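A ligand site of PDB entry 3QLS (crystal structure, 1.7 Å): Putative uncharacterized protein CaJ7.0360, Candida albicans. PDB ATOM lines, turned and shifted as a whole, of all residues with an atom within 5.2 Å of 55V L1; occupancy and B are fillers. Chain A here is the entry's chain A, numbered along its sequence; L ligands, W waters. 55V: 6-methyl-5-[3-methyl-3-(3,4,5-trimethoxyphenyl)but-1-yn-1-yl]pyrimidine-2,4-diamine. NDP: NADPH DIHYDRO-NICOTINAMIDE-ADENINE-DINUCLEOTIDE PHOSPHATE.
Water W3 bridges the side-chain hydroxyl of Ser 61 and an oxygen (O2D) of NDP L2.
N3 of 55V L1 sits at hydrogen-bond distance from OE1 of Glu 32 (2.7 Å).
The backbone carbonyl oxygen (O) of Ile 112 is in hydrogen-bond range of a nitrogen (N1G) of 55V L1 (2.9 Å).
O of Ile 9 is in hydrogen-bond range of N1G of 55V L1 (3.1 Å).
The side-chain hydroxyl (OH) of Tyr 118 is in hydrogen-bond range of a nitrogen (N1G) of 55V L1 (3.2 Å).
N of Ala 11 sits at hydrogen-bond distance from O7N of NDP L2, 2.8 Å away.
The backbone carbonyl oxygen (O) of Ala 11 lies within hydrogen-bond range of a nitrogen (N7N) of NDP L2 (2.9 Å).
N of Thr 58 sits at hydrogen-bond distance from O2A of NDP L2.
OG1 of Thr 58 is in hydrogen-bond range of O2A of NDP L2 (2.6 Å).
The side-chain carboxylate (OE2) of Glu 32 is in hydrogen-bond range of the side-chain hydroxyl (OG1) of Thr 133, at 2.7 Å.
The backbone carbonyl oxygen (O) of Ile 112 is in hydrogen-bond range of the side-chain hydroxyl (OH) of Tyr 118 (3.2 Å).
O of Ile 9 sits at hydrogen-bond distance from OH of Tyr 118 (2.7 Å).
N of Ile 9 sits at hydrogen-bond distance from O of Ile 111 (3.0 Å).
N of Gly 113 is in hydrogen-bond range of OH of Tyr 118 (3.5 Å).
The backbone carbonyl oxygen of Thr 58 lies within hydrogen-bond range of the side-chain hydroxyl of Ser 61, at 2.6 Å.
O of Val 10 is in hydrogen-bond range of N of Thr 133.
The backbone NH (N) of Val 10 is in hydrogen-bond range of the backbone carbonyl oxygen (O) of Leu 131 (3.0 Å).
C of Val 10 touches N1Z of 55V L1 (3.4 Å).
Ala 11 touches 55V L1.
Met 25 touches 55V L1.
Phe 36 touches 55V L1.
Thr 58 touches 55V L1 (CG2 to C1X, 3.8 Å).
O of Ser 61 touches C1U of 55V L1, at 3.4 Å.
Ile 62 touches 55V L1 (CG2 to C1W, 3.8 Å).
CD of Pro 63 touches C1W of 55V L1, 3.7 Å away.
Leu 69 touches 55V L1 (CD2 to C1P, 3.6 Å).
Thr 133 touches 55V L1.
Hydrophobic or aromatic side chains that line 55V L1: Ile 9, Ala 11, Met 25, Phe 36, Ile 62, Pro 63, Leu 69 and Ile 112.
Within 4 Å of 55V L1: Ile 9, Val 10, Ala 11, Met 25, Glu 32, Phe 36, Thr 58, Ser 61, Ile 62, Pro 63, Leu 69, Ile 112, Tyr 118 and Thr 133.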
ATOM      1  N   ILE A   9     -27.245  -8.147 -13.254  1.00  0.00           N
ATOM      2  CA  ILE A   9     -26.213  -7.134 -12.989  1.00  0.00           C
ATOM      3  C   ILE A   9     -26.575  -5.832 -13.686  1.00  0.00           C
ATOM      4  O   ILE A   9     -26.846  -5.813 -14.896  1.00  0.00           O
ATOM      5  CB  ILE A   9     -24.783  -7.647 -13.382  1.00  0.00           C
ATOM      6  CG1 ILE A   9     -23.713  -6.616 -12.993  1.00  0.00           C
ATOM      7  CG2 ILE A   9     -24.726  -8.011 -14.859  1.00  0.00           C
ATOM      8  CD1 ILE A   9     -22.304  -7.224 -12.824  1.00  0.00           C
ATOM      9  N   VAL A  10     -26.589  -4.743 -12.916  1.00  0.00           N
ATOM     10  CA  VAL A  10     -27.102  -3.459 -13.386  1.00  0.00           C
ATOM     11  C   VAL A  10     -26.516  -2.322 -12.527  1.00  0.00           C
ATOM     12  O   VAL A  10     -26.160  -2.537 -11.359  1.00  0.00           O
ATOM     13  CB  VAL A  10     -28.685  -3.417 -13.338  1.00  0.00           C
ATOM     14  CG1 VAL A  10     -29.202  -3.501 -11.901  1.00  0.00           C
ATOM     15  CG2 VAL A  10     -29.215  -2.177 -14.036  1.00  0.00           C
ATOM     16  N   ALA A  11     -26.383  -1.143 -13.133  1.00  0.00           N
ATOM     17  CA  ALA A  11     -26.084   0.100 -12.400  1.00  0.00           C
ATOM     18  C   ALA A  11     -27.256   1.071 -12.523  1.00  0.00           C
ATOM     19  O   ALA A  11     -27.698   1.405 -13.638  1.00  0.00           O
ATOM     20  CB  ALA A  11     -24.798   0.735 -12.928  1.00  0.00           C
ATOM     21  N   MET A  25     -26.793   5.093 -22.034  1.00  0.00           N
ATOM     22  CA  MET A  25     -26.491   5.211 -20.602  1.00  0.00           C
ATOM     23  C   MET A  25     -26.265   6.684 -20.237  1.00  0.00           C
ATOM     24  O   MET A  25     -25.559   7.398 -20.957  1.00  0.00           O
ATOM     25  CB  MET A  25     -25.252   4.378 -20.257  1.00  0.00           C
ATOM     26  CG  MET A  25     -25.321   3.645 -18.928  1.00  0.00           C
ATOM     27  SD  MET A  25     -24.198   2.235 -18.881  1.00  0.00           S
ATOM     28  CE  MET A  25     -25.201   0.986 -19.677  1.00  0.00           C
ATOM     29  N   GLU A  32     -16.778   1.470 -12.766  1.00  0.00           N
ATOM     30  CA  GLU A  32     -17.987   0.641 -12.784  1.00  0.00           C
ATOM     31  C   GLU A  32     -17.988  -0.290 -13.997  1.00  0.00           C
ATOM     32  O   GLU A  32     -18.297  -1.484 -13.898  1.00  0.00           O
ATOM     33  CB  GLU A  32     -19.241   1.532 -12.789  1.00  0.00           C
ATOM     34  CG  GLU A  32     -20.466   0.936 -12.089  1.00  0.00           C
ATOM     35  CD  GLU A  32     -21.044  -0.270 -12.818  1.00  0.00           C
ATOM     36  OE1 GLU A  32     -21.142  -0.231 -14.063  1.00  0.00           O
ATOM     37  OE2 GLU A  32     -21.423  -1.263 -12.144  1.00  0.00           O
ATOM     38  N   ILE A  33     -17.650   0.268 -15.164  1.00  0.00           N
ATOM     39  CA  ILE A  33     -17.518  -0.488 -16.386  1.00  0.00           C
ATOM     40  C   ILE A  33     -16.489  -1.637 -16.234  1.00  0.00           C
ATOM     41  O   ILE A  33     -16.746  -2.762 -16.654  1.00  0.00           O
ATOM     42  CB  ILE A  33     -17.150   0.446 -17.586  1.00  0.00           C
ATOM     43  CG1 ILE A  33     -18.326   1.376 -17.916  1.00  0.00           C
ATOM     44  CG2 ILE A  33     -16.717  -0.356 -18.818  1.00  0.00           C
ATOM     45  CD1 ILE A  33     -17.949   2.605 -18.718  1.00  0.00           C
ATOM     46  N   TYR A  35     -15.555  -3.001 -13.380  1.00  0.00           N
ATOM     47  CA  TYR A  35     -16.216  -3.929 -12.446  1.00  0.00           C
ATOM     48  C   TYR A  35     -17.142  -4.887 -13.200  1.00  0.00           C
ATOM     49  O   TYR A  35     -17.071  -6.104 -13.022  1.00  0.00           O
ATOM     50  CB  TYR A  35     -16.992  -3.150 -11.380  1.00  0.00           C
ATOM     51  CG  TYR A  35     -17.843  -4.008 -10.453  1.00  0.00           C
ATOM     52  CD1 TYR A  35     -17.297  -4.606  -9.320  1.00  0.00           C
ATOM     53  CD2 TYR A  35     -19.212  -4.189 -10.702  1.00  0.00           C
ATOM     54  CE1 TYR A  35     -18.066  -5.377  -8.450  1.00  0.00           C
ATOM     55  CE2 TYR A  35     -20.016  -4.968  -9.830  1.00  0.00           C
ATOM     56  CZ  TYR A  35     -19.432  -5.551  -8.712  1.00  0.00           C
ATOM     57  OH  TYR A  35     -20.187  -6.304  -7.838  1.00  0.00           O
ATOM     58  N   PHE A  36     -17.989  -4.315 -14.059  1.00  0.00           N
ATOM     59  CA  PHE A  36     -18.887  -5.111 -14.895  1.00  0.00           C
ATOM     60  C   PHE A  36     -18.113  -6.150 -15.703  1.00  0.00           C
ATOM     61  O   PHE A  36     -18.498  -7.323 -15.767  1.00  0.00           O
ATOM     62  CB  PHE A  36     -19.711  -4.213 -15.814  1.00  0.00           C
ATOM     63  CG  PHE A  36     -20.441  -4.951 -16.878  1.00  0.00           C
ATOM     64  CD1 PHE A  36     -21.629  -5.638 -16.594  1.00  0.00           C
ATOM     65  CD2 PHE A  36     -19.959  -4.966 -18.194  1.00  0.00           C
ATOM     66  CE1 PHE A  36     -22.317  -6.324 -17.580  1.00  0.00           C
ATOM     67  CE2 PHE A  36     -20.638  -5.647 -19.200  1.00  0.00           C
ATOM     68  CZ  PHE A  36     -21.824  -6.342 -18.887  1.00  0.00           C
ATOM     69  N   THR A  58     -30.358  -3.658 -26.147  1.00  0.00           N
ATOM     70  CA  THR A  58     -29.076  -3.547 -25.429  1.00  0.00           C
ATOM     71  C   THR A  58     -27.906  -4.001 -26.298  1.00  0.00           C
ATOM     72  O   THR A  58     -26.879  -3.313 -26.381  1.00  0.00           O
ATOM     73  CB  THR A  58     -29.113  -4.324 -24.090  1.00  0.00           C
ATOM     74  OG1 THR A  58     -29.994  -3.658 -23.179  1.00  0.00           O
ATOM     75  CG2 THR A  58     -27.720  -4.413 -23.458  1.00  0.00           C
ATOM     76  N   SER A  61     -26.999  -1.516 -28.844  1.00  0.00           N
ATOM     77  CA  SER A  61     -26.390  -0.325 -28.227  1.00  0.00           C
ATOM     78  C   SER A  61     -24.867  -0.446 -28.103  1.00  0.00           C
ATOM     79  O   SER A  61     -24.168   0.577 -28.057  1.00  0.00           O
ATOM     80  CB  SER A  61     -27.025  -0.033 -26.854  1.00  0.00           C
ATOM     81  OG  SER A  61     -26.428  -0.814 -25.831  1.00  0.00           O
ATOM     82  N   ILE A  62     -24.362  -1.665 -28.016  1.00  0.00           N
ATOM     83  CA  ILE A  62     -22.913  -1.902 -27.986  1.00  0.00           C
ATOM     84  C   ILE A  62     -22.355  -1.652 -29.393  1.00  0.00           C
ATOM     85  O   ILE A  62     -22.879  -2.190 -30.370  1.00  0.00           O
ATOM     86  CB  ILE A  62     -22.570  -3.347 -27.550  1.00  0.00           C
ATOM     87  CG1 ILE A  62     -23.255  -3.692 -26.230  1.00  0.00           C
ATOM     88  CG2 ILE A  62     -21.041  -3.547 -27.448  1.00  0.00           C
ATOM     89  CD1 ILE A  62     -23.456  -5.187 -26.008  1.00  0.00           C
ATOM     90  N   PRO A  63     -21.301  -0.823 -29.513  1.00  0.00           N
ATOM     91  CA  PRO A  63     -20.693  -0.606 -30.836  1.00  0.00           C
ATOM     92  C   PRO A  63     -20.375  -1.947 -31.497  1.00  0.00           C
ATOM     93  O   PRO A  63     -19.855  -2.848 -30.836  1.00  0.00           O
ATOM     94  CB  PRO A  63     -19.401   0.149 -30.517  1.00  0.00           C
ATOM     95  CG  PRO A  63     -19.717   0.874 -29.252  1.00  0.00           C
ATOM     96  CD  PRO A  63     -20.626  -0.039 -28.465  1.00  0.00           C
ATOM     97  N   PHE A  66     -17.286  -3.886 -30.862  1.00  0.00           N
ATOM     98  CA  PHE A  66     -16.989  -4.263 -29.482  1.00  0.00           C
ATOM     99  C   PHE A  66     -17.964  -5.315 -28.943  1.00  0.00           C
ATOM    100  O   PHE A  66     -17.978  -5.607 -27.738  1.00  0.00           O
ATOM    101  CB  PHE A  66     -16.943  -3.021 -28.589  1.00  0.00           C
ATOM    102  CG  PHE A  66     -15.810  -2.090 -28.913  1.00  0.00           C
ATOM    103  CD1 PHE A  66     -14.497  -2.420 -28.583  1.00  0.00           C
ATOM    104  CD2 PHE A  66     -16.046  -0.908 -29.596  1.00  0.00           C
ATOM    105  CE1 PHE A  66     -13.433  -1.568 -28.907  1.00  0.00           C
ATOM    106  CE2 PHE A  66     -14.999  -0.050 -29.922  1.00  0.00           C
ATOM    107  CZ  PHE A  66     -13.688  -0.385 -29.579  1.00  0.00           C
ATOM    108  N   LEU A  69     -19.207  -9.228 -26.396  1.00  0.00           N
ATOM    109  CA  LEU A  69     -18.329  -8.975 -25.251  1.00  0.00           C
ATOM    110  C   LEU A  69     -17.367 -10.165 -25.096  1.00  0.00           C
ATOM    111  O   LEU A  69     -17.805 -11.306 -24.980  1.00  0.00           O
ATOM    112  CB  LEU A  69     -19.150  -8.755 -23.978  1.00  0.00           C
ATOM    113  CG  LEU A  69     -20.188  -7.616 -24.032  1.00  0.00           C
ATOM    114  CD1 LEU A  69     -20.931  -7.488 -22.711  1.00  0.00           C
ATOM    115  CD2 LEU A  69     -19.536  -6.277 -24.400  1.00  0.00           C
ATOM    116  N   ILE A 111     -27.701 -11.556 -16.417  1.00  0.00           N
ATOM    117  CA  ILE A 111     -28.559 -10.696 -17.234  1.00  0.00           C
ATOM    118  C   ILE A 111     -27.982  -9.304 -17.239  1.00  0.00           C
ATOM    119  O   ILE A 111     -27.858  -8.678 -16.185  1.00  0.00           O
ATOM    120  CB  ILE A 111     -29.990 -10.638 -16.685  1.00  0.00           C
ATOM    121  CG1 ILE A 111     -30.552 -12.054 -16.469  1.00  0.00           C
ATOM    122  CG2 ILE A 111     -30.889  -9.816 -17.596  1.00  0.00           C
ATOM    123  CD1 ILE A 111     -30.404 -12.985 -17.676  1.00  0.00           C
ATOM    124  N   ILE A 112     -27.630  -8.805 -18.415  1.00  0.00           N
ATOM    125  CA  ILE A 112     -26.910  -7.535 -18.508  1.00  0.00           C
ATOM    126  C   ILE A 112     -27.701  -6.378 -19.153  1.00  0.00           C
ATOM    127  O   ILE A 112     -27.137  -5.298 -19.389  1.00  0.00           O
ATOM    128  CB  ILE A 112     -25.516  -7.702 -19.177  1.00  0.00           C
ATOM    129  CG1 ILE A 112     -25.645  -7.930 -20.692  1.00  0.00           C
ATOM    130  CG2 ILE A 112     -24.739  -8.830 -18.514  1.00  0.00           C
ATOM    131  CD1 ILE A 112     -24.318  -7.888 -21.437  1.00  0.00           C
ATOM    132  N   GLY A 113     -28.990  -6.591 -19.397  1.00  0.00           N
ATOM    133  CA  GLY A 113     -29.900  -5.496 -19.804  1.00  0.00           C
ATOM    134  C   GLY A 113     -30.882  -5.903 -20.899  1.00  0.00           C
ATOM    135  O   GLY A 113     -30.833  -7.024 -21.392  1.00  0.00           O
ATOM    136  N   TYR A 118     -34.830  -6.735 -17.716  1.00  0.00           N
ATOM    137  CA  TYR A 118     -34.687  -6.681 -16.252  1.00  0.00           C
ATOM    138  C   TYR A 118     -36.041  -6.797 -15.566  1.00  0.00           C
ATOM    139  O   TYR A 118     -36.188  -7.544 -14.597  1.00  0.00           O
ATOM    140  CB  TYR A 118     -34.070  -5.359 -15.811  1.00  0.00           C
ATOM    141  CG  TYR A 118     -32.581  -5.197 -16.043  1.00  0.00           C
ATOM    142  CD1 TYR A 118     -31.685  -6.244 -15.802  1.00  0.00           C
ATOM    143  CD2 TYR A 118     -32.062  -3.973 -16.445  1.00  0.00           C
ATOM    144  CE1 TYR A 118     -30.294  -6.058 -15.998  1.00  0.00           C
ATOM    145  CE2 TYR A 118     -30.708  -3.787 -16.642  1.00  0.00           C
ATOM    146  CZ  TYR A 118     -29.824  -4.822 -16.415  1.00  0.00           C
ATOM    147  OH  TYR A 118     -28.482  -4.600 -16.606  1.00  0.00           O
ATOM    148  N   LEU A 131     -26.952  -8.049  -8.596  1.00  0.00           N
ATOM    149  CA  LEU A 131     -25.767  -7.252  -8.406  1.00  0.00           C
ATOM    150  C   LEU A 131     -26.064  -5.834  -8.851  1.00  0.00           C
ATOM    151  O   LEU A 131     -26.030  -5.520 -10.046  1.00  0.00           O
ATOM    152  CB  LEU A 131     -24.578  -7.835  -9.196  1.00  0.00           C
ATOM    153  CG  LEU A 131     -24.016  -9.161  -8.702  1.00  0.00           C
ATOM    154  CD1 LEU A 131     -23.169  -9.816  -9.794  1.00  0.00           C
ATOM    155  CD2 LEU A 131     -23.196  -8.959  -7.443  1.00  0.00           C
ATOM    156  N   THR A 133     -25.272  -1.894  -8.723  1.00  0.00           N
ATOM    157  CA  THR A 133     -24.447  -0.750  -8.405  1.00  0.00           C
ATOM    158  C   THR A 133     -25.387   0.416  -8.129  1.00  0.00           C
ATOM    159  O   THR A 133     -26.058   0.909  -9.039  1.00  0.00           O
ATOM    160  CB  THR A 133     -23.465  -0.415  -9.532  1.00  0.00           C
ATOM    161  OG1 THR A 133     -22.635  -1.559  -9.794  1.00  0.00           O
ATOM    162  CG2 THR A 133     -22.566   0.754  -9.119  1.00  0.00           C
HETATM  163  C1P 55V L   1     -18.986  -3.565 -22.148  1.00  0.00           C
HETATM  164  O1O 55V L   1     -19.125  -2.142 -22.161  1.00  0.00           O
HETATM  165  C1N 55V L   1     -20.400  -1.799 -22.532  1.00  0.00           C
HETATM  166  C1M 55V L   1     -21.496  -2.379 -21.896  1.00  0.00           C
HETATM  167  C1Q 55V L   1     -20.595  -0.861 -23.568  1.00  0.00           C
HETATM  168  O1V 55V L   1     -19.523  -0.278 -24.209  1.00  0.00           O
HETATM  169  C1W 55V L   1     -19.060  -1.105 -25.283  1.00  0.00           C
HETATM  170  C1R 55V L   1     -21.891  -0.509 -23.932  1.00  0.00           C
HETATM  171  O1T 55V L   1     -22.063   0.397 -24.953  1.00  0.00           O
HETATM  172  C1U 55V L   1     -23.277   1.175 -24.842  1.00  0.00           C
HETATM  173  C1S 55V L   1     -22.993  -1.102 -23.295  1.00  0.00           C
HETATM  174  C1L 55V L   1     -22.799  -2.032 -22.264  1.00  0.00           C
HETATM  175  C1J 55V L   1     -24.005  -2.688 -21.556  1.00  0.00           C
HETATM  176  C1K 55V L   1     -24.137  -4.140 -22.024  1.00  0.00           C
HETATM  177  C1X 55V L   1     -25.286  -1.922 -21.873  1.00  0.00           C
HETATM  178  C1I 55V L   1     -23.837  -2.691 -20.081  1.00  0.00           C
HETATM  179  C1H 55V L   1     -23.713  -2.734 -18.855  1.00  0.00           C
HETATM  180  C5  55V L   1     -23.601  -2.775 -17.422  1.00  0.00           C
HETATM  181  C4  55V L   1     -22.664  -1.983 -16.747  1.00  0.00           C
HETATM  182  C1Y 55V L   1     -21.738  -1.023 -17.499  1.00  0.00           C
HETATM  183  N3  55V L   1     -22.588  -2.050 -15.409  1.00  0.00           N
HETATM  184  C2  55V L   1     -23.368  -2.888 -14.705  1.00  0.00           C
HETATM  185  N1Z 55V L   1     -23.265  -2.920 -13.382  1.00  0.00           N
HETATM  186  N1  55V L   1     -24.278  -3.667 -15.325  1.00  0.00           N
HETATM  187  C6  55V L   1     -24.413  -3.637 -16.657  1.00  0.00           C
HETATM  188  N1G 55V L   1     -25.314  -4.419 -17.244  1.00  0.00           N
HETATM  189  PA  NDP L   2     -33.836  -4.225 -23.943  1.00  0.00           P
HETATM  190  O1A NDP L   2     -34.329  -4.795 -22.667  1.00  0.00           O
HETATM  191  O2A NDP L   2     -32.361  -4.246 -24.025  1.00  0.00           O
HETATM  192  O5B NDP L   2     -34.433  -4.998 -25.192  1.00  0.00           O
HETATM  193  C5B NDP L   2     -35.819  -5.117 -25.358  1.00  0.00           C
HETATM  194  C4B NDP L   2     -36.015  -6.127 -26.458  1.00  0.00           C
HETATM  195  O4B NDP L   2     -35.694  -7.424 -25.996  1.00  0.00           O
HETATM  196  C3B NDP L   2     -37.441  -6.205 -26.947  1.00  0.00           C
HETATM  197  O3B NDP L   2     -37.722  -5.169 -27.859  1.00  0.00           O
HETATM  198  C2B NDP L   2     -37.451  -7.594 -27.538  1.00  0.00           C
HETATM  199  O2B NDP L   2     -36.748  -7.605 -28.771  1.00  0.00           O
HETATM  200  C1B NDP L   2     -36.582  -8.372 -26.573  1.00  0.00           C
HETATM  201  N9A NDP L   2     -37.431  -8.992 -25.528  1.00  0.00           N
HETATM  202  C8A NDP L   2     -38.024  -8.379 -24.456  1.00  0.00           C
HETATM  203  N7A NDP L   2     -38.728  -9.309 -23.769  1.00  0.00           N
HETATM  204  C5A NDP L   2     -38.602 -10.503 -24.399  1.00  0.00           C
HETATM  205  C6A NDP L   2     -39.107 -11.773 -24.138  1.00  0.00           C
HETATM  206  N6A NDP L   2     -39.886 -12.002 -23.075  1.00  0.00           N
HETATM  207  N1A NDP L   2     -38.795 -12.817 -24.986  1.00  0.00           N
HETATM  208  C2A NDP L   2     -37.983 -12.588 -26.087  1.00  0.00           C
HETATM  209  N3A NDP L   2     -37.488 -11.328 -26.341  1.00  0.00           N
HETATM  210  C4A NDP L   2     -37.794 -10.302 -25.508  1.00  0.00           C
HETATM  211  O3  NDP L   2     -34.424  -2.769 -24.177  1.00  0.00           O
HETATM  212  PN  NDP L   2     -34.788  -1.504 -23.257  1.00  0.00           P
HETATM  213  O1N NDP L   2     -34.975  -0.362 -24.198  1.00  0.00           O
HETATM  214  O2N NDP L   2     -35.866  -1.873 -22.317  1.00  0.00           O
HETATM  215  O5D NDP L   2     -33.425  -1.241 -22.427  1.00  0.00           O
HETATM  216  C5D NDP L   2     -32.355  -0.550 -23.039  1.00  0.00           C
HETATM  217  C4D NDP L   2     -31.942   0.612 -22.148  1.00  0.00           C
HETATM  218  O4D NDP L   2     -31.419   0.109 -20.908  1.00  0.00           O
HETATM  219  C3D NDP L   2     -30.854   1.448 -22.781  1.00  0.00           C
HETATM  220  O3D NDP L   2     -31.102   2.807 -22.457  1.00  0.00           O
HETATM  221  C2D NDP L   2     -29.596   0.987 -22.092  1.00  0.00           C
HETATM  222  O2D NDP L   2     -28.606   1.990 -22.045  1.00  0.00           O
HETATM  223  C1D NDP L   2     -30.126   0.664 -20.705  1.00  0.00           C
HETATM  224  N1N NDP L   2     -29.249  -0.251 -19.959  1.00  0.00           N
HETATM  225  C2N NDP L   2     -28.751   0.195 -18.768  1.00  0.00           C
HETATM  226  C3N NDP L   2     -27.912  -0.598 -18.011  1.00  0.00           C
HETATM  227  C7N NDP L   2     -27.310  -0.026 -16.771  1.00  0.00           C
HETATM  228  O7N NDP L   2     -26.592  -0.874 -15.920  1.00  0.00           O
HETATM  229  N7N NDP L   2     -27.471   1.274 -16.519  1.00  0.00           N
HETATM  230  C4N NDP L   2     -27.560  -1.872 -18.477  1.00  0.00           C
HETATM  231  C5N NDP L   2     -28.067  -2.315 -19.701  1.00  0.00           C
HETATM  232  C6N NDP L   2     -28.907  -1.491 -20.443  1.00  0.00           C
HETATM  233  P2B NDP L   2     -37.492  -7.475 -30.194  1.00  0.00           P
HETATM  234  O1X NDP L   2     -36.469  -7.735 -31.257  1.00  0.00           O
HETATM  235  O2X NDP L   2     -38.605  -8.474 -30.255  1.00  0.00           O
HETATM  236  O3X NDP L   2     -38.022  -6.063 -30.322  1.00  0.00           O
HETATM  237  O   HOH W   1     -16.937  -3.592 -19.478  1.00  0.00           O
HETATM  238  O   HOH W   2     -17.368  -5.949 -20.568  1.00  0.00           O
HETATM  239  O   HOH W   3     -26.333   0.876 -23.627  1.00  0.00           O
HETATM  240  O   HOH W   4     -25.377   3.378 -24.969  1.00  0.00           O
